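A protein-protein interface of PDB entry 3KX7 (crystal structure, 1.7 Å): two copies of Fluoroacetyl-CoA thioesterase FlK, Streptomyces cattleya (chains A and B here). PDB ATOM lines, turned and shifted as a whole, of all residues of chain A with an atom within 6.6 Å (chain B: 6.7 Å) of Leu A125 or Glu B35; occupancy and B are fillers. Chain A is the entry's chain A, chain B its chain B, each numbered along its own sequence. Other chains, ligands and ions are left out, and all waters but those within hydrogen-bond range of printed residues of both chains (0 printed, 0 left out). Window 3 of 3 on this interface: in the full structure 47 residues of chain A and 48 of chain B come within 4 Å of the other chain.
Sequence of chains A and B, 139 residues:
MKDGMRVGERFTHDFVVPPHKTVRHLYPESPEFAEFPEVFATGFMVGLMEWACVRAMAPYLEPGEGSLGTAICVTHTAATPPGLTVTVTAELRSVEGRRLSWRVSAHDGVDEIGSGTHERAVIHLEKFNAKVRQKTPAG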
ATOM      1  N   GLY A  64      34.397  -9.874 -22.143  1.00  0.00           N
ATOM      2  CA  GLY A  64      33.901 -10.548 -23.343  1.00  0.00           C
ATOM      3  C   GLY A  64      33.942 -12.071 -23.286  1.00  0.00           C
ATOM      4  O   GLY A  64      33.611 -12.743 -24.269  1.00  0.00           O
ATOM      5  N   GLU A  65      34.358 -12.618 -22.145  1.00  0.00           N
ATOM      6  CA  GLU A  65      34.380 -14.073 -21.955  1.00  0.00           C
ATOM      7  C   GLU A  65      33.207 -14.521 -21.106  1.00  0.00           C
ATOM      8  O   GLU A  65      32.655 -13.738 -20.329  1.00  0.00           O
ATOM      9  CB  GLU A  65      35.687 -14.539 -21.295  1.00  0.00           C
ATOM     10  CG  GLU A  65      36.912 -14.587 -22.215  1.00  0.00           C
ATOM     11  CD  GLU A  65      38.146 -15.184 -21.542  1.00  0.00           C
ATOM     12  OE1 GLU A  65      38.296 -15.042 -20.309  1.00  0.00           O
ATOM     13  OE2 GLU A  65      38.972 -15.812 -22.243  1.00  0.00           O
ATOM     14  N   GLY A  66      32.835 -15.787 -21.265  1.00  0.00           N
ATOM     15  CA  GLY A  66      31.851 -16.435 -20.405  1.00  0.00           C
ATOM     16  C   GLY A  66      32.281 -17.868 -20.203  1.00  0.00           C
ATOM     17  O   GLY A  66      33.462 -18.190 -20.350  1.00  0.00           O
ATOM     18  N   SER A  67      31.331 -18.746 -19.876  1.00  0.00           N
ATOM     19  CA  SER A  67      31.626 -20.174 -19.776  1.00  0.00           C
ATOM     20  C   SER A  67      30.393 -21.003 -20.129  1.00  0.00           C
ATOM     21  O   SER A  67      29.273 -20.480 -20.134  1.00  0.00           O
ATOM     22  CB  SER A  67      32.127 -20.544 -18.375  1.00  0.00           C
ATOM     23  OG  SER A  67      31.084 -20.452 -17.411  1.00  0.00           O
ATOM     24  N   ILE A 123      34.580 -19.611 -22.573  1.00  0.00           N
ATOM     25  CA  ILE A 123      34.313 -19.385 -23.980  1.00  0.00           C
ATOM     26  C   ILE A 123      34.437 -17.906 -24.262  1.00  0.00           C
ATOM     27  O   ILE A 123      34.333 -17.079 -23.350  1.00  0.00           O
ATOM     28  CB  ILE A 123      32.914 -19.936 -24.447  1.00  0.00           C
ATOM     29  CG1 ILE A 123      31.767 -19.343 -23.622  1.00  0.00           C
ATOM     30  CG2 ILE A 123      32.893 -21.465 -24.422  1.00  0.00           C
ATOM     31  CD1 ILE A 123      30.420 -19.362 -24.340  1.00  0.00           C
ATOM     32  N   HIS A 124      34.684 -17.574 -25.520  1.00  0.00           N
ATOM     33  CA  HIS A 124      34.579 -16.187 -25.974  1.00  0.00           C
ATOM     34  C   HIS A 124      33.166 -15.952 -26.476  1.00  0.00           C
ATOM     35  O   HIS A 124      32.776 -16.508 -27.506  1.00  0.00           O
ATOM     36  N   LEU A 125      32.418 -15.118 -25.750  1.00  0.00           N
ATOM     37  CA  LEU A 125      30.968 -14.970 -25.927  1.00  0.00           C
ATOM     38  C   LEU A 125      30.527 -14.576 -27.325  1.00  0.00           C
ATOM     39  O   LEU A 125      29.526 -15.086 -27.829  1.00  0.00           O
ATOM     40  CB  LEU A 125      30.392 -13.977 -24.909  1.00  0.00           C
ATOM     41  CG  LEU A 125      30.298 -14.456 -23.460  1.00  0.00           C
ATOM     42  CD1 LEU A 125      30.003 -13.287 -22.535  1.00  0.00           C
ATOM     43  CD2 LEU A 125      29.247 -15.565 -23.293  1.00  0.00           C
ATOM     44  N   GLU A 126      31.276 -13.674 -27.950  1.00  0.00           N
ATOM     45  CA  GLU A 126      30.888 -13.118 -29.244  1.00  0.00           C
ATOM     46  C   GLU A 126      31.274 -14.064 -30.369  1.00  0.00           C
ATOM     47  O   GLU A 126      30.569 -14.162 -31.372  1.00  0.00           O
ATOM     48  CB  GLU A 126      31.513 -11.735 -29.454  1.00  0.00           C
ATOM     49  CG  GLU A 126      31.404 -10.797 -28.238  1.00  0.00           C
ATOM     50  CD  GLU A 126      32.304 -11.211 -27.067  1.00  0.00           C
ATOM     51  OE1 GLU A 126      33.358 -11.859 -27.298  1.00  0.00           O
ATOM     52  OE2 GLU A 126      31.947 -10.885 -25.915  1.00  0.00           O
ATOM     53  N   LYS A 127      32.386 -14.770 -30.197  1.00  0.00           N
ATOM     54  CA  LYS A 127      32.733 -15.833 -31.123  1.00  0.00           C
ATOM     55  C   LYS A 127      31.656 -16.907 -31.058  1.00  0.00           C
ATOM     56  O   LYS A 127      31.164 -17.364 -32.095  1.00  0.00           O
ATOM     57  CB  LYS A 127      34.096 -16.442 -30.785  1.00  0.00           C
ATOM     58  CG  LYS A 127      34.508 -17.572 -31.731  1.00  0.00           C
ATOM     59  CD  LYS A 127      35.990 -17.507 -32.125  1.00  0.00           C
ATOM     60  CE  LYS A 127      36.379 -16.168 -32.772  1.00  0.00           C
ATOM     61  NZ  LYS A 127      36.909 -15.186 -31.772  1.00  0.00           N
ATOM     62  N   PHE A 128      31.287 -17.290 -29.835  1.00  0.00           N
ATOM     63  CA  PHE A 128      30.359 -18.392 -29.627  1.00  0.00           C
ATOM     64  C   PHE A 128      28.981 -18.091 -30.200  1.00  0.00           C
ATOM     65  O   PHE A 128      28.413 -18.922 -30.913  1.00  0.00           O
ATOM     66  CB  PHE A 128      30.266 -18.785 -28.146  1.00  0.00           C
ATOM     67  CG  PHE A 128      29.405 -20.005 -27.898  1.00  0.00           C
ATOM     68  CD1 PHE A 128      29.920 -21.291 -28.081  1.00  0.00           C
ATOM     69  CD2 PHE A 128      28.079 -19.861 -27.504  1.00  0.00           C
ATOM     70  CE1 PHE A 128      29.125 -22.419 -27.864  1.00  0.00           C
ATOM     71  CE2 PHE A 128      27.272 -20.982 -27.286  1.00  0.00           C
ATOM     72  CZ  PHE A 128      27.797 -22.261 -27.465  1.00  0.00           C
ATOM     73  N   ASN A 129      28.456 -16.905 -29.897  1.00  0.00           N
ATOM     74  CA  ASN A 129      27.166 -16.477 -30.422  1.00  0.00           C
ATOM     75  C   ASN A 129      27.066 -16.499 -31.947  1.00  0.00           C
ATOM     76  O   ASN A 129      26.000 -16.780 -32.486  1.00  0.00           O
ATOM     77  CB  ASN A 129      26.772 -15.110 -29.863  1.00  0.00           C
ATOM     78  CG  ASN A 129      26.504 -15.155 -28.372  1.00  0.00           C
ATOM     79  OD1 ASN A 129      26.142 -16.199 -27.826  1.00  0.00           O
ATOM     80  ND2 ASN A 129      26.686 -14.023 -27.701  1.00  0.00           N
ATOM     81  N   ALA A 130      28.178 -16.226 -32.629  1.00  0.00           N
ATOM     82  CA  ALA A 130      28.226 -16.292 -34.094  1.00  0.00           C
ATOM     83  C   ALA A 130      28.119 -17.728 -34.600  1.00  0.00           C
ATOM     84  O   ALA A 130      27.339 -18.011 -35.513  1.00  0.00           O
ATOM     85  CB  ALA A 130      29.491 -15.630 -34.618  1.00  0.00           C
ATOM     86  N   ARG A 133      24.578 -19.113 -34.017  1.00  0.00           N
ATOM     87  CA  ARG A 133      23.591 -18.539 -34.935  1.00  0.00           C
ATOM     88  C   ARG A 133      23.512 -19.312 -36.267  1.00  0.00           C
ATOM     89  O   ARG A 133      22.515 -19.211 -36.985  1.00  0.00           O
ATOM     90  CB  ARG A 133      23.825 -17.027 -35.135  1.00  0.00           C
ATOM     91  CG  ARG A 133      23.525 -16.209 -33.856  1.00  0.00           C
ATOM     92  CD  ARG A 133      23.845 -14.712 -33.953  1.00  0.00           C
ATOM     93  NE  ARG A 133      24.278 -14.139 -32.667  1.00  0.00           N
ATOM     94  CZ  ARG A 133      23.468 -13.664 -31.718  1.00  0.00           C
ATOM     95  NH1 ARG A 133      22.147 -13.683 -31.879  1.00  0.00           N
ATOM     96  NH2 ARG A 133      23.982 -13.167 -30.597  1.00  0.00           N
ATOM     97  N   ARG B  24      19.188 -18.737 -18.770  1.00  0.00           N
ATOM     98  CA  ARG B  24      18.597 -17.570 -18.141  1.00  0.00           C
ATOM     99  C   ARG B  24      17.136 -17.831 -17.784  1.00  0.00           C
ATOM    100  O   ARG B  24      16.606 -17.231 -16.849  1.00  0.00           O
ATOM    101  CB  ARG B  24      18.815 -16.284 -18.951  1.00  0.00           C
ATOM    102  CG  ARG B  24      18.030 -16.163 -20.219  1.00  0.00           C
ATOM    103  CD  ARG B  24      18.212 -14.778 -20.818  1.00  0.00           C
ATOM    104  NE  ARG B  24      17.089 -14.458 -21.690  1.00  0.00           N
ATOM    105  CZ  ARG B  24      17.036 -14.786 -22.972  1.00  0.00           C
ATOM    106  NH1 ARG B  24      18.062 -15.411 -23.507  1.00  0.00           N
ATOM    107  NH2 ARG B  24      15.978 -14.468 -23.713  1.00  0.00           N
ATOM    108  N   PRO B  31      21.010 -12.896 -11.800  1.00  0.00           N
ATOM    109  CA  PRO B  31      21.541 -11.844 -12.656  1.00  0.00           C
ATOM    110  C   PRO B  31      22.827 -12.329 -13.292  1.00  0.00           C
ATOM    111  O   PRO B  31      23.136 -11.990 -14.427  1.00  0.00           O
ATOM    112  CB  PRO B  31      21.861 -10.701 -11.681  1.00  0.00           C
ATOM    113  CG  PRO B  31      21.187 -11.029 -10.411  1.00  0.00           C
ATOM    114  CD  PRO B  31      20.957 -12.504 -10.383  1.00  0.00           C
ATOM    115  N   GLU B  32      23.551 -13.163 -12.562  1.00  0.00           N
ATOM    116  CA  GLU B  32      24.817 -13.673 -13.032  1.00  0.00           C
ATOM    117  C   GLU B  32      24.715 -14.514 -14.317  1.00  0.00           C
ATOM    118  O   GLU B  32      25.742 -14.822 -14.906  1.00  0.00           O
ATOM    119  CB  GLU B  32      25.546 -14.424 -11.907  1.00  0.00           C
ATOM    120  CG  GLU B  32      26.004 -13.526 -10.763  1.00  0.00           C
ATOM    121  CD  GLU B  32      24.922 -13.318  -9.716  1.00  0.00           C
ATOM    122  OE1 GLU B  32      24.941 -12.269  -9.016  1.00  0.00           O
ATOM    123  OE2 GLU B  32      24.038 -14.198  -9.595  1.00  0.00           O
ATOM    124  N   PHE B  33      23.487 -14.878 -14.730  1.00  0.00           N
ATOM    125  CA  PHE B  33      23.227 -15.599 -16.013  1.00  0.00           C
ATOM    126  C   PHE B  33      22.778 -14.674 -17.163  1.00  0.00           C
ATOM    127  O   PHE B  33      22.477 -15.141 -18.269  1.00  0.00           O
ATOM    128  CB  PHE B  33      22.142 -16.691 -15.851  1.00  0.00           C
ATOM    129  CG  PHE B  33      22.617 -17.968 -15.193  1.00  0.00           C
ATOM    130  CD1 PHE B  33      21.768 -18.662 -14.325  1.00  0.00           C
ATOM    131  CD2 PHE B  33      23.873 -18.491 -15.451  1.00  0.00           C
ATOM    132  CE1 PHE B  33      22.171 -19.837 -13.711  1.00  0.00           C
ATOM    133  CE2 PHE B  33      24.290 -19.672 -14.844  1.00  0.00           C
ATOM    134  CZ  PHE B  33      23.434 -20.344 -13.961  1.00  0.00           C
ATOM    135  N   ALA B  34      22.734 -13.369 -16.901  1.00  0.00           N
ATOM    136  CA  ALA B  34      22.051 -12.415 -17.783  1.00  0.00           C
ATOM    137  C   ALA B  34      22.509 -12.449 -19.243  1.00  0.00           C
ATOM    138  O   ALA B  34      21.683 -12.397 -20.158  1.00  0.00           O
ATOM    139  CB  ALA B  34      22.151 -10.990 -17.220  1.00  0.00           C
ATOM    140  N   GLU B  35      23.820 -12.550 -19.451  1.00  0.00           N
ATOM    141  CA  GLU B  35      24.386 -12.497 -20.799  1.00  0.00           C
ATOM    142  C   GLU B  35      24.910 -13.842 -21.283  1.00  0.00           C
ATOM    143  O   GLU B  35      25.847 -13.914 -22.088  1.00  0.00           O
ATOM    144  CB  GLU B  35      25.472 -11.418 -20.890  1.00  0.00           C
ATOM    145  CG  GLU B  35      24.932  -9.980 -20.861  1.00  0.00           C
ATOM    146  CD  GLU B  35      23.882  -9.704 -21.939  1.00  0.00           C
ATOM    147  OE1 GLU B  35      22.751  -9.296 -21.587  1.00  0.00           O
ATOM    148  OE2 GLU B  35      24.184  -9.898 -23.138  1.00  0.00           O
ATOM    149  N   PHE B  36      24.304 -14.914 -20.790  1.00  0.00           N
ATOM    150  CA  PHE B  36      24.624 -16.233 -21.291  1.00  0.00           C
ATOM    151  C   PHE B  36      24.031 -16.415 -22.686  1.00  0.00           C
ATOM    152  O   PHE B  36      22.990 -15.820 -23.006  1.00  0.00           O
ATOM    153  CB  PHE B  36      24.111 -17.311 -20.329  1.00  0.00           C
ATOM    154  CG  PHE B  36      25.168 -17.843 -19.394  1.00  0.00           C
ATOM    155  CD1 PHE B  36      25.559 -19.186 -19.442  1.00  0.00           C
ATOM    156  CD2 PHE B  36      25.773 -17.005 -18.465  1.00  0.00           C
ATOM    157  CE1 PHE B  36      26.542 -19.685 -18.564  1.00  0.00           C
ATOM    158  CE2 PHE B  36      26.747 -17.483 -17.589  1.00  0.00           C
ATOM    159  CZ  PHE B  36      27.132 -18.832 -17.638  1.00  0.00           C
ATOM    160  N   PRO B  37      24.689 -17.225 -23.527  1.00  0.00           N
ATOM    161  CA  PRO B  37      24.168 -17.444 -24.873  1.00  0.00           C
ATOM    162  C   PRO B  37      22.829 -18.176 -24.837  1.00  0.00           C
ATOM    163  O   PRO B  37      22.557 -18.924 -23.884  1.00  0.00           O
ATOM    164  CB  PRO B  37      25.211 -18.346 -25.526  1.00  0.00           C
ATOM    165  CG  PRO B  37      26.425 -18.277 -24.662  1.00  0.00           C
ATOM    166  CD  PRO B  37      25.929 -17.990 -23.282  1.00  0.00           C
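O of Gly A64 lies within hydrogen-bond range of N of Leu A125, at 3.0 Å. The backbone carbonyl oxygen (O) of Asn A129 lies close to the guanidinium group (NE) of Arg A133 (3.2 Å). The side-chain amide nitrogen (ND2) of Asn A129 is in hydrogen-bond range of the backbone carbonyl oxygen (O) of Leu A125 (3.0 Å).
Among the printed residues, pairs that only touch across the chains: Ser A67 with Phe B36 (3.2 Å), Leu A125 with Glu B35 (3.97 Å), Phe A128 with Pro B37 (3.6 Å) and Asn A129 with Pro B37 (3.3 Å).
Printed residues of chain B within 4 Å of Ser A67: Phe B36 (3.2 Å). Of chain B, only Glu B35 comes within 4 Å of Leu A125. Printed residues of chain B within 4 Å of Phe A128: Pro B37 (3.6 Å). Of the printed residues of chain B, Asn A129 touches Pro B37 (3.3 Å). Glu B32 touches none of the printed residues of chain A. Of the printed residues of chain A, Phe B36 touches Ser A67. Of the printed residues of chain A, Pro B37 touches Phe A128 and Asn A129. The nearest residue of chain A that does not touch Glu B35 is Asn A129 (5.7 Å).
Printed residues of chain A that touch a printed residue of chain B: Ser A67, Leu A125, Phe A128 and Asn A129. Hydrophobic or aromatic side chains of chain A that line the printed part of chain B: Leu A125 and Phe A128. Among the printed residues, 4 pairs touch across the chains.
No position is printed for both chains.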
